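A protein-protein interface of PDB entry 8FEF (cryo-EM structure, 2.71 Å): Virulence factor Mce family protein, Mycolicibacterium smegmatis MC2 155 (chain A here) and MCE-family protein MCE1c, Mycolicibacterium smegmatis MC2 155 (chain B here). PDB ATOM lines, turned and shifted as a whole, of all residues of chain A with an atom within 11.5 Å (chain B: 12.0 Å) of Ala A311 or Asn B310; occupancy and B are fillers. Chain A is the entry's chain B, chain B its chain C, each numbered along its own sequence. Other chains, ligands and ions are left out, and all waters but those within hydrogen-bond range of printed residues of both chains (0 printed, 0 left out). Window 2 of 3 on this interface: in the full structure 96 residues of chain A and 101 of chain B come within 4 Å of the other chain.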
ATOM      1  N   PHE A 307     -16.838 -27.069 -22.218  1.00  0.00           N
ATOM      2  CA  PHE A 307     -17.931 -27.641 -21.449  1.00  0.00           C
ATOM      3  C   PHE A 307     -18.785 -26.529 -20.845  1.00  0.00           C
ATOM      4  O   PHE A 307     -18.402 -25.357 -20.815  1.00  0.00           O
ATOM      5  CB  PHE A 307     -17.402 -28.548 -20.340  1.00  0.00           C
ATOM      6  CG  PHE A 307     -17.100 -29.944 -20.787  1.00  0.00           C
ATOM      7  CD1 PHE A 307     -18.091 -30.908 -20.795  1.00  0.00           C
ATOM      8  CD2 PHE A 307     -15.826 -30.301 -21.182  1.00  0.00           C
ATOM      9  CE1 PHE A 307     -17.819 -32.197 -21.200  1.00  0.00           C
ATOM     10  CE2 PHE A 307     -15.549 -31.589 -21.587  1.00  0.00           C
ATOM     11  CZ  PHE A 307     -16.547 -32.538 -21.597  1.00  0.00           C
ATOM     12  N   ASN A 308     -19.958 -26.906 -20.352  1.00  0.00           N
ATOM     13  CA  ASN A 308     -20.848 -25.982 -19.659  1.00  0.00           C
ATOM     14  C   ASN A 308     -20.947 -26.412 -18.202  1.00  0.00           C
ATOM     15  O   ASN A 308     -21.529 -27.457 -17.897  1.00  0.00           O
ATOM     16  CB  ASN A 308     -22.227 -25.942 -20.310  1.00  0.00           C
ATOM     17  CG  ASN A 308     -22.233 -25.176 -21.608  1.00  0.00           C
ATOM     18  OD1 ASN A 308     -22.223 -23.947 -21.611  1.00  0.00           O
ATOM     19  ND2 ASN A 308     -22.258 -25.895 -22.722  1.00  0.00           N
ATOM     20  N   PHE A 309     -20.377 -25.610 -17.311  1.00  0.00           N
ATOM     21  CA  PHE A 309     -20.453 -25.838 -15.876  1.00  0.00           C
ATOM     22  C   PHE A 309     -21.289 -24.740 -15.237  1.00  0.00           C
ATOM     23  O   PHE A 309     -21.228 -23.579 -15.653  1.00  0.00           O
ATOM     24  CB  PHE A 309     -19.061 -25.871 -15.242  1.00  0.00           C
ATOM     25  CG  PHE A 309     -18.360 -27.193 -15.369  1.00  0.00           C
ATOM     26  CD1 PHE A 309     -18.839 -28.174 -16.216  1.00  0.00           C
ATOM     27  CD2 PHE A 309     -17.223 -27.456 -14.626  1.00  0.00           C
ATOM     28  CE1 PHE A 309     -18.191 -29.388 -16.327  1.00  0.00           C
ATOM     29  CE2 PHE A 309     -16.573 -28.669 -14.733  1.00  0.00           C
ATOM     30  CZ  PHE A 309     -17.058 -29.635 -15.584  1.00  0.00           C
ATOM     31  N   TYR A 310     -22.077 -25.112 -14.231  1.00  0.00           N
ATOM     32  CA  TYR A 310     -22.896 -24.164 -13.484  1.00  0.00           C
ATOM     33  C   TYR A 310     -22.590 -24.339 -12.007  1.00  0.00           C
ATOM     34  O   TYR A 310     -22.738 -25.440 -11.468  1.00  0.00           O
ATOM     35  CB  TYR A 310     -24.386 -24.383 -13.761  1.00  0.00           C
ATOM     36  CG  TYR A 310     -25.269 -23.234 -13.339  1.00  0.00           C
ATOM     37  CD1 TYR A 310     -25.721 -23.120 -12.033  1.00  0.00           C
ATOM     38  CD2 TYR A 310     -25.658 -22.265 -14.251  1.00  0.00           C
ATOM     39  CE1 TYR A 310     -26.530 -22.070 -11.645  1.00  0.00           C
ATOM     40  CE2 TYR A 310     -26.469 -21.214 -13.873  1.00  0.00           C
ATOM     41  CZ  TYR A 310     -26.902 -21.122 -12.569  1.00  0.00           C
ATOM     42  OH  TYR A 310     -27.708 -20.076 -12.189  1.00  0.00           O
ATOM     43  N   ALA A 311     -22.167 -23.260 -11.354  1.00  0.00           N
ATOM     44  CA  ALA A 311     -21.806 -23.283  -9.939  1.00  0.00           C
ATOM     45  C   ALA A 311     -22.983 -22.745  -9.134  1.00  0.00           C
ATOM     46  O   ALA A 311     -23.199 -21.533  -9.067  1.00  0.00           O
ATOM     47  CB  ALA A 311     -20.543 -22.469  -9.689  1.00  0.00           C
ATOM     48  N   CYS A 312     -23.746 -23.651  -8.522  1.00  0.00           N
ATOM     49  CA  CYS A 312     -24.894 -23.230  -7.728  1.00  0.00           C
ATOM     50  C   CYS A 312     -24.483 -22.802  -6.327  1.00  0.00           C
ATOM     51  O   CYS A 312     -25.072 -21.875  -5.760  1.00  0.00           O
ATOM     52  CB  CYS A 312     -25.934 -24.347  -7.659  1.00  0.00           C
ATOM     53  SG  CYS A 312     -27.127 -24.274  -9.005  1.00  0.00           S
ATOM     54  N   ASP A 313     -23.481 -23.461  -5.755  1.00  0.00           N
ATOM     55  CA  ASP A 313     -22.984 -23.131  -4.426  1.00  0.00           C
ATOM     56  C   ASP A 313     -21.465 -23.172  -4.442  1.00  0.00           C
ATOM     57  O   ASP A 313     -20.874 -24.234  -4.656  1.00  0.00           O
ATOM     58  CB  ASP A 313     -23.547 -24.091  -3.374  1.00  0.00           C
ATOM     59  CG  ASP A 313     -23.592 -25.527  -3.857  1.00  0.00           C
ATOM     60  OD1 ASP A 313     -23.204 -25.777  -5.016  1.00  0.00           O
ATOM     61  OD2 ASP A 313     -24.021 -26.405  -3.081  1.00  0.00           O
ATOM     62  N   LEU A 314     -20.837 -22.022  -4.217  1.00  0.00           N
ATOM     63  CA  LEU A 314     -19.385 -21.924  -4.159  1.00  0.00           C
ATOM     64  C   LEU A 314     -18.996 -21.602  -2.724  1.00  0.00           C
ATOM     65  O   LEU A 314     -19.509 -20.643  -2.130  1.00  0.00           O
ATOM     66  CB  LEU A 314     -18.842 -20.886  -5.148  1.00  0.00           C
ATOM     67  CG  LEU A 314     -18.926 -19.371  -4.946  1.00  0.00           C
ATOM     68  CD1 LEU A 314     -17.650 -18.836  -4.315  1.00  0.00           C
ATOM     69  CD2 LEU A 314     -19.213 -18.669  -6.265  1.00  0.00           C
ATOM     70  N   THR A 315     -18.124 -22.439  -2.160  1.00  0.00           N
ATOM     71  CA  THR A 315     -17.670 -22.318  -0.785  1.00  0.00           C
ATOM     72  C   THR A 315     -16.162 -22.510  -0.733  1.00  0.00           C
ATOM     73  O   THR A 315     -15.616 -23.364  -1.437  1.00  0.00           O
ATOM     74  CB  THR A 315     -18.321 -23.380   0.109  1.00  0.00           C
ATOM     75  OG1 THR A 315     -17.982 -24.676  -0.392  1.00  0.00           O
ATOM     76  CG2 THR A 315     -19.827 -23.264   0.078  1.00  0.00           C
ATOM     77  N   LEU A 316     -15.499 -21.721   0.105  1.00  0.00           N
ATOM     78  CA  LEU A 316     -14.046 -21.715   0.193  1.00  0.00           C
ATOM     79  C   LEU A 316     -13.592 -22.556   1.377  1.00  0.00           C
ATOM     80  O   LEU A 316     -14.150 -22.458   2.472  1.00  0.00           O
ATOM     81  CB  LEU A 316     -13.507 -20.289   0.325  1.00  0.00           C
ATOM     82  CG  LEU A 316     -13.094 -19.567  -0.961  1.00  0.00           C
ATOM     83  CD1 LEU A 316     -14.157 -19.669  -2.043  1.00  0.00           C
ATOM     84  CD2 LEU A 316     -12.776 -18.109  -0.666  1.00  0.00           C
ATOM     85  N   ARG A 331     -18.609 -20.577   3.555  1.00  0.00           N
ATOM     86  CA  ARG A 331     -19.620 -20.634   2.510  1.00  0.00           C
ATOM     87  C   ARG A 331     -19.868 -19.239   1.956  1.00  0.00           C
ATOM     88  O   ARG A 331     -20.180 -18.312   2.710  1.00  0.00           O
ATOM     89  CB  ARG A 331     -20.918 -21.230   3.066  1.00  0.00           C
ATOM     90  CG  ARG A 331     -22.061 -21.385   2.070  1.00  0.00           C
ATOM     91  CD  ARG A 331     -23.094 -20.271   2.193  1.00  0.00           C
ATOM     92  NE  ARG A 331     -23.708 -20.224   3.516  1.00  0.00           N
ATOM     93  CZ  ARG A 331     -23.421 -19.321   4.444  1.00  0.00           C
ATOM     94  NH1 ARG A 331     -22.538 -18.361   4.225  1.00  0.00           N
ATOM     95  NH2 ARG A 331     -24.037 -19.384   5.621  1.00  0.00           N
ATOM     96  N   ILE A 332     -19.732 -19.094   0.636  1.00  0.00           N
ATOM     97  CA  ILE A 332     -19.899 -17.793   0.002  1.00  0.00           C
ATOM     98  C   ILE A 332     -21.275 -17.691  -0.643  1.00  0.00           C
ATOM     99  O   ILE A 332     -22.079 -16.832  -0.266  1.00  0.00           O
ATOM    100  CB  ILE A 332     -18.784 -17.514  -1.022  1.00  0.00           C
ATOM    101  CG1 ILE A 332     -17.423 -17.507  -0.327  1.00  0.00           C
ATOM    102  CG2 ILE A 332     -19.025 -16.183  -1.712  1.00  0.00           C
ATOM    103  CD1 ILE A 332     -16.315 -16.909  -1.162  1.00  0.00           C
ATOM    104  N   THR A 333     -21.564 -18.556  -1.621  1.00  0.00           N
ATOM    105  CA  THR A 333     -22.840 -18.484  -2.322  1.00  0.00           C
ATOM    106  C   THR A 333     -23.527 -19.840  -2.351  1.00  0.00           C
ATOM    107  O   THR A 333     -22.879 -20.886  -2.462  1.00  0.00           O
ATOM    108  CB  THR A 333     -22.701 -17.995  -3.775  1.00  0.00           C
ATOM    109  OG1 THR A 333     -22.056 -19.002  -4.562  1.00  0.00           O
ATOM    110  CG2 THR A 333     -21.913 -16.697  -3.853  1.00  0.00           C
ATOM    111  N   THR A 334     -24.856 -19.796  -2.281  1.00  0.00           N
ATOM    112  CA  THR A 334     -25.715 -20.960  -2.432  1.00  0.00           C
ATOM    113  C   THR A 334     -26.962 -20.537  -3.196  1.00  0.00           C
ATOM    114  O   THR A 334     -27.338 -19.362  -3.205  1.00  0.00           O
ATOM    115  CB  THR A 334     -26.114 -21.568  -1.078  1.00  0.00           C
ATOM    116  OG1 THR A 334     -26.533 -20.524  -0.190  1.00  0.00           O
ATOM    117  CG2 THR A 334     -24.958 -22.333  -0.452  1.00  0.00           C
ATOM    118  N   GLN A 335     -27.602 -21.504  -3.843  1.00  0.00           N
ATOM    119  CA  GLN A 335     -28.853 -21.256  -4.563  1.00  0.00           C
ATOM    120  C   GLN A 335     -29.962 -22.095  -3.948  1.00  0.00           C
ATOM    121  O   GLN A 335     -29.943 -23.333  -4.082  1.00  0.00           O
ATOM    122  CB  GLN A 335     -28.708 -21.564  -6.053  1.00  0.00           C
ATOM    123  CG  GLN A 335     -29.919 -21.154  -6.879  1.00  0.00           C
ATOM    124  CD  GLN A 335     -29.694 -21.297  -8.373  1.00  0.00           C
ATOM    125  OE1 GLN A 335     -30.452 -20.759  -9.180  1.00  0.00           O
ATOM    126  NE2 GLN A 335     -28.649 -22.022  -8.747  1.00  0.00           N
ATOM    127  N   PRO A 336     -30.931 -21.487  -3.255  1.00  0.00           N
ATOM    128  CA  PRO A 336     -31.992 -22.276  -2.612  1.00  0.00           C
ATOM    129  C   PRO A 336     -32.915 -22.962  -3.607  1.00  0.00           C
ATOM    130  O   PRO A 336     -33.146 -24.172  -3.519  1.00  0.00           O
ATOM    131  CB  PRO A 336     -32.753 -21.233  -1.781  1.00  0.00           C
ATOM    132  CG  PRO A 336     -31.829 -20.057  -1.676  1.00  0.00           C
ATOM    133  CD  PRO A 336     -31.048 -20.054  -2.948  1.00  0.00           C
ATOM    134  N   SER A 337     -33.445 -22.200  -4.559  1.00  0.00           N
ATOM    135  CA  SER A 337     -34.404 -22.713  -5.523  1.00  0.00           C
ATOM    136  C   SER A 337     -34.017 -22.265  -6.923  1.00  0.00           C
ATOM    137  O   SER A 337     -33.360 -21.238  -7.106  1.00  0.00           O
ATOM    138  CB  SER A 337     -35.832 -22.245  -5.205  1.00  0.00           C
ATOM    139  OG  SER A 337     -36.249 -22.708  -3.932  1.00  0.00           O
ATOM    140  N   GLY A 338     -34.436 -23.051  -7.910  1.00  0.00           N
ATOM    141  CA  GLY A 338     -34.119 -22.766  -9.294  1.00  0.00           C
ATOM    142  C   GLY A 338     -33.769 -24.024 -10.057  1.00  0.00           C
ATOM    143  O   GLY A 338     -34.418 -25.060  -9.888  1.00  0.00           O
ATOM    144  N   ARG A 339     -32.742 -23.947 -10.906  1.00  0.00           N
ATOM    145  CA  ARG A 339     -32.329 -25.115 -11.671  1.00  0.00           C
ATOM    146  C   ARG A 339     -31.712 -26.192 -10.792  1.00  0.00           C
ATOM    147  O   ARG A 339     -31.677 -27.357 -11.199  1.00  0.00           O
ATOM    148  CB  ARG A 339     -31.340 -24.710 -12.764  1.00  0.00           C
ATOM    149  CG  ARG A 339     -30.102 -24.022 -12.241  1.00  0.00           C
ATOM    150  CD  ARG A 339     -29.057 -23.847 -13.325  1.00  0.00           C
ATOM    151  NE  ARG A 339     -28.435 -25.105 -13.720  1.00  0.00           N
ATOM    152  CZ  ARG A 339     -28.614 -25.691 -14.895  1.00  0.00           C
ATOM    153  NH1 ARG A 339     -29.397 -25.161 -15.818  1.00  0.00           N
ATOM    154  NH2 ARG A 339     -27.976 -26.827 -15.156  1.00  0.00           N
ATOM    155  N   CYS A 340     -31.223 -25.834  -9.607  1.00  0.00           N
ATOM    156  CA  CYS A 340     -30.602 -26.782  -8.684  1.00  0.00           C
ATOM    157  C   CYS A 340     -31.453 -26.855  -7.421  1.00  0.00           C
ATOM    158  O   CYS A 340     -31.202 -26.155  -6.438  1.00  0.00           O
ATOM    159  CB  CYS A 340     -29.168 -26.383  -8.373  1.00  0.00           C
ATOM    160  SG  CYS A 340     -28.921 -24.626  -8.124  1.00  0.00           S
ATOM    161  N   THR A 341     -32.464 -27.716  -7.461  1.00  0.00           N
ATOM    162  CA  THR A 341     -33.244 -28.112  -6.306  1.00  0.00           C
ATOM    163  C   THR A 341     -33.304 -29.633  -6.280  1.00  0.00           C
ATOM    164  O   THR A 341     -33.309 -30.263  -7.345  1.00  0.00           O
ATOM    165  CB  THR A 341     -34.660 -27.518  -6.361  1.00  0.00           C
ATOM    166  OG1 THR A 341     -35.486 -28.132  -5.367  1.00  0.00           O
ATOM    167  CG2 THR A 341     -35.279 -27.727  -7.731  1.00  0.00           C
ATOM    168  N   VAL B 306     -13.847 -25.129 -19.807  1.00  0.00           N
ATOM    169  CA  VAL B 306     -15.110 -25.059 -19.083  1.00  0.00           C
ATOM    170  C   VAL B 306     -15.587 -23.616 -19.059  1.00  0.00           C
ATOM    171  O   VAL B 306     -14.792 -22.689 -18.876  1.00  0.00           O
ATOM    172  CB  VAL B 306     -14.991 -25.611 -17.648  1.00  0.00           C
ATOM    173  CG1 VAL B 306     -14.958 -27.111 -17.667  1.00  0.00           C
ATOM    174  CG2 VAL B 306     -13.748 -25.072 -16.967  1.00  0.00           C
ATOM    175  N   MET B 307     -16.886 -23.425 -19.255  1.00  0.00           N
ATOM    176  CA  MET B 307     -17.508 -22.112 -19.157  1.00  0.00           C
ATOM    177  C   MET B 307     -18.281 -22.039 -17.848  1.00  0.00           C
ATOM    178  O   MET B 307     -19.255 -22.773 -17.656  1.00  0.00           O
ATOM    179  CB  MET B 307     -18.434 -21.844 -20.342  1.00  0.00           C
ATOM    180  CG  MET B 307     -18.919 -20.407 -20.410  1.00  0.00           C
ATOM    181  SD  MET B 307     -20.051 -20.089 -21.771  1.00  0.00           S
ATOM    182  CE  MET B 307     -20.144 -18.304 -21.710  1.00  0.00           C
ATOM    183  N   LEU B 308     -17.849 -21.153 -16.958  1.00  0.00           N
ATOM    184  CA  LEU B 308     -18.471 -20.972 -15.653  1.00  0.00           C
ATOM    185  C   LEU B 308     -19.391 -19.759 -15.736  1.00  0.00           C
ATOM    186  O   LEU B 308     -18.922 -18.618 -15.752  1.00  0.00           O
ATOM    187  CB  LEU B 308     -17.411 -20.790 -14.571  1.00  0.00           C
ATOM    188  CG  LEU B 308     -16.324 -21.865 -14.514  1.00  0.00           C
ATOM    189  CD1 LEU B 308     -15.168 -21.416 -13.639  1.00  0.00           C
ATOM    190  CD2 LEU B 308     -16.899 -23.170 -14.002  1.00  0.00           C
ATOM    191  N   VAL B 309     -20.701 -20.009 -15.793  1.00  0.00           N
ATOM    192  CA  VAL B 309     -21.672 -18.925 -15.889  1.00  0.00           C
ATOM    193  C   VAL B 309     -21.820 -18.173 -14.572  1.00  0.00           C
ATOM    194  O   VAL B 309     -22.380 -17.069 -14.543  1.00  0.00           O
ATOM    195  CB  VAL B 309     -22.992 -19.547 -16.409  1.00  0.00           C
ATOM    196  CG1 VAL B 309     -24.146 -18.550 -16.456  1.00  0.00           C
ATOM    197  CG2 VAL B 309     -22.772 -20.161 -17.778  1.00  0.00           C
ATOM    198  N   ASN B 310     -21.249 -18.695 -13.492  1.00  0.00           N
ATOM    199  CA  ASN B 310     -21.277 -18.008 -12.207  1.00  0.00           C
ATOM    200  C   ASN B 310     -19.873 -17.611 -11.758  1.00  0.00           C
ATOM    201  O   ASN B 310     -19.271 -18.269 -10.910  1.00  0.00           O
ATOM    202  CB  ASN B 310     -21.943 -18.888 -11.153  1.00  0.00           C
ATOM    203  CG  ASN B 310     -23.364 -19.246 -11.520  1.00  0.00           C
ATOM    204  OD1 ASN B 310     -24.022 -18.524 -12.266  1.00  0.00           O
ATOM    205  ND2 ASN B 310     -23.845 -20.365 -11.002  1.00  0.00           N
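O of Phe A307 is in hydrogen-bond range of N of Met B307, at 2.9 Å. The backbone NH (N) of Phe A309 is in hydrogen-bond range of the backbone carbonyl oxygen (O) of Met B307. N of Ala A311 sits close to ND2 of Asn B310.
SG of Cys A312 forms a disulfide with SG of Cys A340 (2.0 Å).
Among the printed residues, pairs that only touch across the chains: Phe A307 with Val B306 (3.7 Å), Phe A309 with Val B306 (3.7 Å), Phe A309 with Leu B308 (3.7 Å), Phe A309 with Val B309 (3.6 Å) and Tyr A310 with Asn B310 (3.2 Å).
Ala A311 touches just one residue of chain B: Asn B310 (2.4 Å). Asn B310 touches just these residues of chain A: Tyr A310 (3.2 Å) and Ala A311 (2.4 Å). No residue of chain B comes within 4 Å of Cys A312. Of the printed residues of chain A, Leu B308 touches Phe A309 (3.7 Å). Val B309 touches just one residue of chain A: Phe A309. Of the printed residues of chain A, Met B307 touches Phe A307 and Phe A309. Printed residues of chain B within 4 Å of Phe A309: Val B306, Met B307, Leu B308 and Val B309. Printed residues of chain A within 4 Å of Val B306: Phe A307 and Phe A309. Leu A316 touches none of the printed residues of chain B.
Hydrophobic or aromatic side chains of chain B within 4 Å of the printed part of chain A: Val B306, Met B307 and Leu B308. Of the 21 printed residues of chain A, 4 touch a printed residue of chain B. Printed residues of chain A that touch a printed residue of chain B: Phe A307, Phe A309, Tyr A310 and Ala A311. Among the printed residues, 8 pairs touch across the chains. Among the printed residues, no Asp or Glu carboxylate lies within 4 Å of a Lys or Arg side-chain nitrogen of the other chain.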
